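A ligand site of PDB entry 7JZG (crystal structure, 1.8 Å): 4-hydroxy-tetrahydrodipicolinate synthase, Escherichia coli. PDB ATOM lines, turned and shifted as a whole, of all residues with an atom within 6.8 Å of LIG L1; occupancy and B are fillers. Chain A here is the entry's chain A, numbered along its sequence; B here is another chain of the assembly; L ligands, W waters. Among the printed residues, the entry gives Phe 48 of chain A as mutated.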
ATOM      1  N   VAL A  42     -37.079   7.030  -4.680  1.00  0.00           N
ATOM      2  CA  VAL A  42     -35.611   7.264  -4.922  1.00  0.00           C
ATOM      3  C   VAL A  42     -35.326   8.763  -4.680  1.00  0.00           C
ATOM      4  O   VAL A  42     -34.725   9.416  -5.485  1.00  0.00           O
ATOM      5  CB  VAL A  42     -35.141   6.814  -6.326  1.00  0.00           C
ATOM      6  CG1 VAL A  42     -33.612   6.740  -6.333  1.00  0.00           C
ATOM      7  CG2 VAL A  42     -35.659   5.397  -6.687  1.00  0.00           C
ATOM      8  N   GLU A  47     -31.808   6.334  -1.375  1.00  0.00           N
ATOM      9  CA  GLU A  47     -30.502   6.027  -1.882  1.00  0.00           C
ATOM     10  C   GLU A  47     -30.258   6.426  -3.343  1.00  0.00           C
ATOM     11  O   GLU A  47     -29.537   5.725  -4.084  1.00  0.00           O
ATOM     12  CB  GLU A  47     -30.068   4.632  -1.553  1.00  0.00           C
ATOM     13  CG  GLU A  47     -29.684   4.426  -0.058  1.00  0.00           C
ATOM     14  CD  GLU A  47     -29.483   2.989   0.303  1.00  0.00           C
ATOM     15  OE1 GLU A  47     -30.538   2.321   0.636  1.00  0.00           O
ATOM     16  OE2 GLU A  47     -28.293   2.496   0.276  1.00  0.00           O
ATOM     17  N   PHE A  48     -30.779   7.562  -3.747  1.00  0.00           N
ATOM     18  CA  PHE A  48     -30.467   7.996  -5.079  1.00  0.00           C
ATOM     19  C   PHE A  48     -29.001   8.092  -5.444  1.00  0.00           C
ATOM     20  O   PHE A  48     -28.655   7.742  -6.569  1.00  0.00           O
ATOM     21  CB  PHE A  48     -31.180   9.233  -5.575  1.00  0.00           C
ATOM     22  CG  PHE A  48     -30.538  10.549  -5.238  1.00  0.00           C
ATOM     23  CD1 PHE A  48     -29.437  11.008  -5.870  1.00  0.00           C
ATOM     24  CD2 PHE A  48     -31.123  11.335  -4.266  1.00  0.00           C
ATOM     25  CE1 PHE A  48     -28.845  12.207  -5.583  1.00  0.00           C
ATOM     26  CE2 PHE A  48     -30.616  12.582  -3.955  1.00  0.00           C
ATOM     27  CZ  PHE A  48     -29.453  13.018  -4.595  1.00  0.00           C
ATOM     28  N   ALA A  49     -28.186   8.429  -4.484  1.00  0.00           N
ATOM     29  CA  ALA A  49     -26.741   8.560  -4.836  1.00  0.00           C
ATOM     30  C   ALA A  49     -26.051   7.258  -5.237  1.00  0.00           C
ATOM     31  O   ALA A  49     -25.132   7.282  -6.094  1.00  0.00           O
ATOM     32  CB  ALA A  49     -26.035   9.126  -3.615  1.00  0.00           C
ATOM     33  N   THR A  50     -26.531   6.138  -4.724  1.00  0.00           N
ATOM     34  CA  THR A  50     -25.826   4.899  -5.054  1.00  0.00           C
ATOM     35  C   THR A  50     -26.535   3.929  -6.045  1.00  0.00           C
ATOM     36  O   THR A  50     -25.985   2.825  -6.226  1.00  0.00           O
ATOM     37  CB  THR A  50     -25.541   4.122  -3.783  1.00  0.00           C
ATOM     38  OG1 THR A  50     -26.721   3.883  -3.068  1.00  0.00           O
ATOM     39  CG2 THR A  50     -24.588   4.934  -2.864  1.00  0.00           C
ATOM     40  N   LEU A  51     -27.612   4.384  -6.668  1.00  0.00           N
ATOM     41  CA  LEU A  51     -28.216   3.670  -7.783  1.00  0.00           C
ATOM     42  C   LEU A  51     -27.733   4.326  -9.021  1.00  0.00           C
ATOM     43  O   LEU A  51     -27.661   5.553  -9.054  1.00  0.00           O
ATOM     44  CB  LEU A  51     -29.717   3.783  -7.635  1.00  0.00           C
ATOM     45  CG  LEU A  51     -30.334   3.195  -6.416  1.00  0.00           C
ATOM     46  CD1 LEU A  51     -31.844   3.422  -6.420  1.00  0.00           C
ATOM     47  CD2 LEU A  51     -30.050   1.728  -6.270  1.00  0.00           C
ATOM     48  N   ASN A  52     -27.412   3.519 -10.040  1.00  0.00           N
ATOM     49  CA  ASN A  52     -27.211   4.094 -11.388  1.00  0.00           C
ATOM     50  C   ASN A  52     -28.507   4.532 -11.968  1.00  0.00           C
ATOM     51  O   ASN A  52     -29.593   4.312 -11.407  1.00  0.00           O
ATOM     52  CB  ASN A  52     -26.322   3.243 -12.255  1.00  0.00           C
ATOM     53  CG  ASN A  52     -26.977   1.984 -12.720  1.00  0.00           C
ATOM     54  OD1 ASN A  52     -28.141   2.030 -13.028  1.00  0.00           O
ATOM     55  ND2 ASN A  52     -26.212   0.850 -12.782  1.00  0.00           N
ATOM     56  N   HIS A  53     -28.456   5.291 -13.073  1.00  0.00           N
ATOM     57  CA  HIS A  53     -29.702   5.875 -13.611  1.00  0.00           C
ATOM     58  C   HIS A  53     -30.673   4.784 -14.042  1.00  0.00           C
ATOM     59  O   HIS A  53     -31.866   4.917 -13.891  1.00  0.00           O
ATOM     60  CB  HIS A  53     -29.467   6.760 -14.855  1.00  0.00           C
ATOM     61  CG  HIS A  53     -29.316   8.208 -14.505  1.00  0.00           C
ATOM     62  ND1 HIS A  53     -29.424   9.224 -15.440  1.00  0.00           N
ATOM     63  CD2 HIS A  53     -29.066   8.790 -13.314  1.00  0.00           C
ATOM     64  CE1 HIS A  53     -29.212  10.379 -14.836  1.00  0.00           C
ATOM     65  NE2 HIS A  53     -29.016  10.148 -13.546  1.00  0.00           N
ATOM     66  N   ASP A  54     -30.147   3.700 -14.600  1.00  0.00           N
ATOM     67  CA  ASP A  54     -31.082   2.587 -14.960  1.00  0.00           C
ATOM     68  C   ASP A  54     -31.727   1.925 -13.781  1.00  0.00           C
ATOM     69  O   ASP A  54     -32.928   1.612 -13.774  1.00  0.00           O
ATOM     70  CB  ASP A  54     -30.356   1.534 -15.806  1.00  0.00           C
ATOM     71  CG  ASP A  54     -30.030   2.066 -17.194  1.00  0.00           C
ATOM     72  OD1 ASP A  54     -30.824   2.752 -17.841  1.00  0.00           O
ATOM     73  OD2 ASP A  54     -28.943   1.793 -17.625  1.00  0.00           O
ATOM     74  N   HIS A  56     -32.193   3.276 -10.868  1.00  0.00           N
ATOM     75  CA  HIS A  56     -33.064   4.325 -10.257  1.00  0.00           C
ATOM     76  C   HIS A  56     -34.409   4.281 -11.003  1.00  0.00           C
ATOM     77  O   HIS A  56     -35.476   4.152 -10.412  1.00  0.00           O
ATOM     78  CB  HIS A  56     -32.330   5.638 -10.486  1.00  0.00           C
ATOM     79  CG  HIS A  56     -33.017   6.858 -10.002  1.00  0.00           C
ATOM     80  ND1 HIS A  56     -32.260   7.958  -9.545  1.00  0.00           N
ATOM     81  CD2 HIS A  56     -34.315   7.225  -9.949  1.00  0.00           C
ATOM     82  CE1 HIS A  56     -33.092   8.922  -9.202  1.00  0.00           C
ATOM     83  NE2 HIS A  56     -34.344   8.521  -9.440  1.00  0.00           N
ATOM     84  N   ALA A  57     -34.311   4.271 -12.329  1.00  0.00           N
ATOM     85  CA  ALA A  57     -35.549   4.235 -13.115  1.00  0.00           C
ATOM     86  C   ALA A  57     -36.313   2.933 -12.848  1.00  0.00           C
ATOM     87  O   ALA A  57     -37.543   2.938 -12.749  1.00  0.00           O
ATOM     88  CB  ALA A  57     -35.284   4.502 -14.562  1.00  0.00           C
ATOM     89  N   GLY A  78     -33.430  14.494  -9.232  1.00  0.00           N
ATOM     90  CA  GLY A  78     -32.353  15.506  -9.118  1.00  0.00           C
ATOM     91  C   GLY A  78     -31.045  15.003  -9.695  1.00  0.00           C
ATOM     92  O   GLY A  78     -30.781  13.786  -9.806  1.00  0.00           O
ATOM     93  N   ALA A  79     -30.202  16.000 -10.045  1.00  0.00           N
ATOM     94  CA  ALA A  79     -28.819  15.718 -10.462  1.00  0.00           C
ATOM     95  C   ALA A  79     -28.031  16.990 -10.280  1.00  0.00           C
ATOM     96  O   ALA A  79     -28.613  18.096 -10.314  1.00  0.00           O
ATOM     97  CB  ALA A  79     -28.685  15.198 -11.868  1.00  0.00           C
ATOM     98  N   ASN A  80     -26.721  16.881 -10.193  1.00  0.00           N
ATOM     99  CA  ASN A  80     -25.942  18.127 -10.101  1.00  0.00           C
ATOM    100  C   ASN A  80     -25.451  18.605 -11.423  1.00  0.00           C
ATOM    101  O   ASN A  80     -24.759  19.637 -11.466  1.00  0.00           O
ATOM    102  CB  ASN A  80     -24.767  18.004  -9.070  1.00  0.00           C
ATOM    103  CG  ASN A  80     -23.784  16.902  -9.459  1.00  0.00           C
ATOM    104  OD1 ASN A  80     -23.959  16.231 -10.482  1.00  0.00           O
ATOM    105  ND2 ASN A  80     -22.673  16.787  -8.694  1.00  0.00           N
ATOM    106  N   GLU A  84     -27.952  15.940 -17.047  1.00  0.00           N
ATOM    107  CA  GLU A  84     -28.295  14.716 -16.422  1.00  0.00           C
ATOM    108  C   GLU A  84     -29.647  14.723 -15.761  1.00  0.00           C
ATOM    109  O   GLU A  84     -30.415  13.759 -15.811  1.00  0.00           O
ATOM    110  CB  GLU A  84     -27.148  14.462 -15.415  1.00  0.00           C
ATOM    111  CG  GLU A  84     -27.195  13.256 -14.714  1.00  0.00           C
ATOM    112  CD  GLU A  84     -25.950  13.029 -13.756  1.00  0.00           C
ATOM    113  OE1 GLU A  84     -26.021  12.024 -13.009  1.00  0.00           O
ATOM    114  OE2 GLU A  84     -24.951  13.798 -13.694  1.00  0.00           O
ATOM    115  N   LEU A  88     -32.805  12.261 -16.761  1.00  0.00           N
ATOM    116  CA  LEU A  88     -33.531  11.519 -15.833  1.00  0.00           C
ATOM    117  C   LEU A  88     -35.014  11.832 -15.824  1.00  0.00           C
ATOM    118  O   LEU A  88     -35.861  10.942 -15.796  1.00  0.00           O
ATOM    119  CB  LEU A  88     -32.908  11.647 -14.437  1.00  0.00           C
ATOM    120  CG  LEU A  88     -33.321  10.870 -13.292  1.00  0.00           C
ATOM    121  CD1 LEU A  88     -33.284   9.372 -13.485  1.00  0.00           C
ATOM    122  CD2 LEU A  88     -32.361  11.216 -12.076  1.00  0.00           C
ATOM    123  N   TYR A 106     -25.661  19.506  -6.073  1.00  0.00           N
ATOM    124  CA  TYR A 106     -24.792  19.204  -4.985  1.00  0.00           C
ATOM    125  C   TYR A 106     -23.327  19.225  -5.468  1.00  0.00           C
ATOM    126  O   TYR A 106     -23.029  18.961  -6.585  1.00  0.00           O
ATOM    127  CB  TYR A 106     -25.112  17.920  -4.274  1.00  0.00           C
ATOM    128  CG  TYR A 106     -25.495  16.843  -5.196  1.00  0.00           C
ATOM    129  CD1 TYR A 106     -24.551  15.946  -5.743  1.00  0.00           C
ATOM    130  CD2 TYR A 106     -26.839  16.733  -5.621  1.00  0.00           C
ATOM    131  CE1 TYR A 106     -24.951  14.998  -6.687  1.00  0.00           C
ATOM    132  CE2 TYR A 106     -27.207  15.792  -6.539  1.00  0.00           C
ATOM    133  CZ  TYR A 106     -26.272  14.915  -7.051  1.00  0.00           C
ATOM    134  OH  TYR A 106     -26.618  13.967  -7.991  1.00  0.00           O
ATOM    135  N   HIS B  53     -19.060   9.804 -17.387  1.00  0.00           N
ATOM    136  CA  HIS B  53     -17.849   8.981 -17.182  1.00  0.00           C
ATOM    137  C   HIS B  53     -17.054   8.905 -18.433  1.00  0.00           C
ATOM    138  O   HIS B  53     -15.810   8.993 -18.424  1.00  0.00           O
ATOM    139  CB  HIS B  53     -18.162   7.579 -16.596  1.00  0.00           C
ATOM    140  CG  HIS B  53     -18.567   7.600 -15.164  1.00  0.00           C
ATOM    141  ND1 HIS B  53     -17.749   7.148 -14.164  1.00  0.00           N
ATOM    142  CD2 HIS B  53     -19.721   7.976 -14.552  1.00  0.00           C
ATOM    143  CE1 HIS B  53     -18.329   7.335 -12.996  1.00  0.00           C
ATOM    144  NE2 HIS B  53     -19.538   7.823 -13.209  1.00  0.00           N
ATOM    145  N   ALA B  79     -16.127   9.592  -6.424  1.00  0.00           N
ATOM    146  CA  ALA B  79     -17.595   9.438  -6.600  1.00  0.00           C
ATOM    147  C   ALA B  79     -18.213   9.311  -5.292  1.00  0.00           C
ATOM    148  O   ALA B  79     -17.595   8.928  -4.311  1.00  0.00           O
ATOM    149  CB  ALA B  79     -17.912   8.199  -7.430  1.00  0.00           C
ATOM    150  N   ASN B  80     -19.508   9.572  -5.242  1.00  0.00           N
ATOM    151  CA  ASN B  80     -20.252   9.359  -4.021  1.00  0.00           C
ATOM    152  C   ASN B  80     -20.874   7.966  -3.817  1.00  0.00           C
ATOM    153  O   ASN B  80     -21.454   7.714  -2.767  1.00  0.00           O
ATOM    154  CB  ASN B  80     -21.325  10.416  -3.759  1.00  0.00           C
ATOM    155  CG  ASN B  80     -22.429  10.430  -4.769  1.00  0.00           C
ATOM    156  OD1 ASN B  80     -22.393   9.737  -5.759  1.00  0.00           O
ATOM    157  ND2 ASN B  80     -23.419  11.309  -4.587  1.00  0.00           N
ATOM    158  N   ALA B  81     -20.630   7.083  -4.773  1.00  0.00           N
ATOM    159  CA  ALA B  81     -20.966   5.689  -4.677  1.00  0.00           C
ATOM    160  C   ALA B  81     -19.707   4.879  -4.833  1.00  0.00           C
ATOM    161  O   ALA B  81     -18.949   5.102  -5.760  1.00  0.00           O
ATOM    162  CB  ALA B  81     -21.993   5.278  -5.759  1.00  0.00           C
ATOM    163  N   GLU B  84     -19.071   3.144  -8.187  1.00  0.00           N
ATOM    164  CA  GLU B  84     -18.804   4.071  -9.206  1.00  0.00           C
ATOM    165  C   GLU B  84     -17.343   4.533  -9.191  1.00  0.00           C
ATOM    166  O   GLU B  84     -16.706   4.719 -10.250  1.00  0.00           O
ATOM    167  CB  GLU B  84     -19.823   5.196  -8.958  1.00  0.00           C
ATOM    168  CG  GLU B  84     -19.963   6.165 -10.024  1.00  0.00           C
ATOM    169  CD  GLU B  84     -21.040   7.308  -9.753  1.00  0.00           C
ATOM    170  OE1 GLU B  84     -22.040   7.124  -8.915  1.00  0.00           O
ATOM    171  OE2 GLU B  84     -20.775   8.416 -10.349  1.00  0.00           O
ATOM    172  N   TYR B 106     -19.983  12.894  -1.527  1.00  0.00           N
ATOM    173  CA  TYR B 106     -20.814  14.104  -1.416  1.00  0.00           C
ATOM    174  C   TYR B 106     -22.293  13.731  -1.372  1.00  0.00           C
ATOM    175  O   TYR B 106     -22.696  12.684  -1.930  1.00  0.00           O
ATOM    176  CB  TYR B 106     -20.530  15.065  -2.575  1.00  0.00           C
ATOM    177  CG  TYR B 106     -20.289  14.433  -3.894  1.00  0.00           C
ATOM    178  CD1 TYR B 106     -21.314  14.213  -4.774  1.00  0.00           C
ATOM    179  CD2 TYR B 106     -19.046  13.997  -4.234  1.00  0.00           C
ATOM    180  CE1 TYR B 106     -21.126  13.562  -5.977  1.00  0.00           C
ATOM    181  CE2 TYR B 106     -18.849  13.363  -5.414  1.00  0.00           C
ATOM    182  CZ  TYR B 106     -19.892  13.157  -6.284  1.00  0.00           C
ATOM    183  OH  TYR B 106     -19.583  12.509  -7.437  1.00  0.00           O
ATOM    184  N   TYR B 107     -23.071  14.557  -0.707  1.00  0.00           N
ATOM    185  CA  TYR B 107     -24.498  14.522  -0.606  1.00  0.00           C
ATOM    186  C   TYR B 107     -24.990  13.453   0.385  1.00  0.00           C
ATOM    187  O   TYR B 107     -25.856  13.749   1.236  1.00  0.00           O
ATOM    188  CB  TYR B 107     -25.157  14.344  -2.029  1.00  0.00           C
ATOM    189  CG  TYR B 107     -26.672  14.447  -1.919  1.00  0.00           C
ATOM    190  CD1 TYR B 107     -27.244  15.682  -1.937  1.00  0.00           C
ATOM    191  CD2 TYR B 107     -27.440  13.356  -1.608  1.00  0.00           C
ATOM    192  CE1 TYR B 107     -28.575  15.873  -1.769  1.00  0.00           C
ATOM    193  CE2 TYR B 107     -28.806  13.506  -1.401  1.00  0.00           C
ATOM    194  CZ  TYR B 107     -29.369  14.797  -1.476  1.00  0.00           C
ATOM    195  OH  TYR B 107     -30.699  15.052  -1.303  1.00  0.00           O
HETATM  196  N1  LIG L   1     -23.831   8.726  -7.762  1.00  0.00           N
HETATM  197  C1  LIG L   1     -24.093   9.977  -8.715  1.00  0.00           C
HETATM  198  C2  LIG L   1     -24.792  11.212  -8.068  1.00  0.00           C
HETATM  199  O1  LIG L   1     -25.164  11.200  -6.864  1.00  0.00           O
HETATM  200  C3  LIG L   1     -25.026   9.541  -9.846  1.00  0.00           C
HETATM  201  C4  LIG L   1     -26.375   8.993  -9.350  1.00  0.00           C
HETATM  202  C5  LIG L   1     -27.303   8.673 -10.546  1.00  0.00           C
HETATM  203  C6  LIG L   1     -28.662   9.160 -10.140  1.00  0.00           C
HETATM  204  N2  LIG L   1     -29.464   8.117  -9.582  1.00  0.00           N
HETATM  205  O2  LIG L   1     -25.141  12.230  -8.780  1.00  0.00           O
HETATM  206  N1  LG2 L   2     -22.874  14.372 -12.121  1.00  0.00           N
HETATM  207  C1  LG2 L   2     -22.549  13.131 -11.208  1.00  0.00           C
HETATM  208  C2  LG2 L   2     -21.706  13.376  -9.907  1.00  0.00           C
HETATM  209  O1  LG2 L   2     -21.442  12.394  -9.145  1.00  0.00           O
HETATM  210  C3  LG2 L   2     -21.773  12.052 -12.034  1.00  0.00           C
HETATM  211  C4  LG2 L   2     -20.394  12.529 -12.598  1.00  0.00           C
HETATM  212  C5  LG2 L   2     -19.596  11.340 -13.115  1.00  0.00           C
HETATM  213  C6  LG2 L   2     -18.358  11.642 -13.969  1.00  0.00           C
HETATM  214  N2  LG2 L   2     -17.383  12.505 -13.390  1.00  0.00           N
HETATM  215  O2  LG2 L   2     -21.213  14.524  -9.656  1.00  0.00           O
HETATM  216  O   HOH W   1     -28.831  11.892 -10.586  1.00  0.00           O
HETATM  217  O   HOH W   2     -24.262   5.504  -8.852  1.00  0.00           O
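The backbone carbonyl oxygen of Leu 51 sits at hydrogen-bond distance from a nitrogen (N2) of LIG L1 (3.2 Å). The side-chain hydroxyl (OH) of Tyr 106 of chain A is in hydrogen-bond range of an oxygen (O2) of LIG L1 (2.4 Å). OE1 of Glu 84 of chain B is in salt-bridge range of N1 of LIG L1 (2.7 Å). A ring nitrogen (ND1) of His 56 lies within hydrogen-bond range of a nitrogen (N2) of LIG L1 (2.8 Å). The side-chain carboxylate (OE2) of Glu 84 of chain A is in salt-bridge range of a nitrogen (N1) of LG2 L2, at 2.7 Å. N2 of LIG L1 is in hydrogen-bond range of O of Phe 48 (3.1 Å). The backbone carbonyl oxygen (O) of Ala 49 is in hydrogen-bond range of a nitrogen (N1) of LIG L1 (2.6 Å). OH of Tyr 106 of chain B is in hydrogen-bond range of O1 of LG2 L2 (2.5 Å). A nitrogen (N1) of LIG L1 lies within hydrogen-bond range of the side-chain amide oxygen (OD1) of Asn 80 of chain B, 2.7 Å away. A nitrogen (N1) of LG2 L2 is in hydrogen-bond range of the side-chain amide oxygen (OD1) of Asn 80 of chain A.
The side-chain carboxylate (OE2) of Glu 84 of chain B is in hydrogen-bond range of a ring nitrogen (NE2) of His 53 of chain B. The backbone carbonyl oxygen (O) of Tyr 106 of chain B lies within hydrogen-bond range of the side-chain amide nitrogen (ND2) of Asn 80 of chain B, 3.1 Å away. The side-chain amide nitrogen of Asn 80 of chain A is in hydrogen-bond range of the backbone carbonyl oxygen of Tyr 106 of chain A (3.0 Å).
CD2 of His 53 of chain A touches C6 of LIG L1 (3.2 Å). Hydrophobic or aromatic side chains that line LIG L1: Ala 49, His 53 of chain A, His 56 and Tyr 106 of chain A. Of the 24 residues printed, 8 come within 4 Å of LIG L1. Along chain A the residues within 4 Å of LIG L1 span positions 48 to 106.
Water W1 bridges the backbone carbonyl oxygen (O) of Gly 78 (2.8 Å) and a ring nitrogen (NE2) of His 53 of chain A (3.4 Å).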
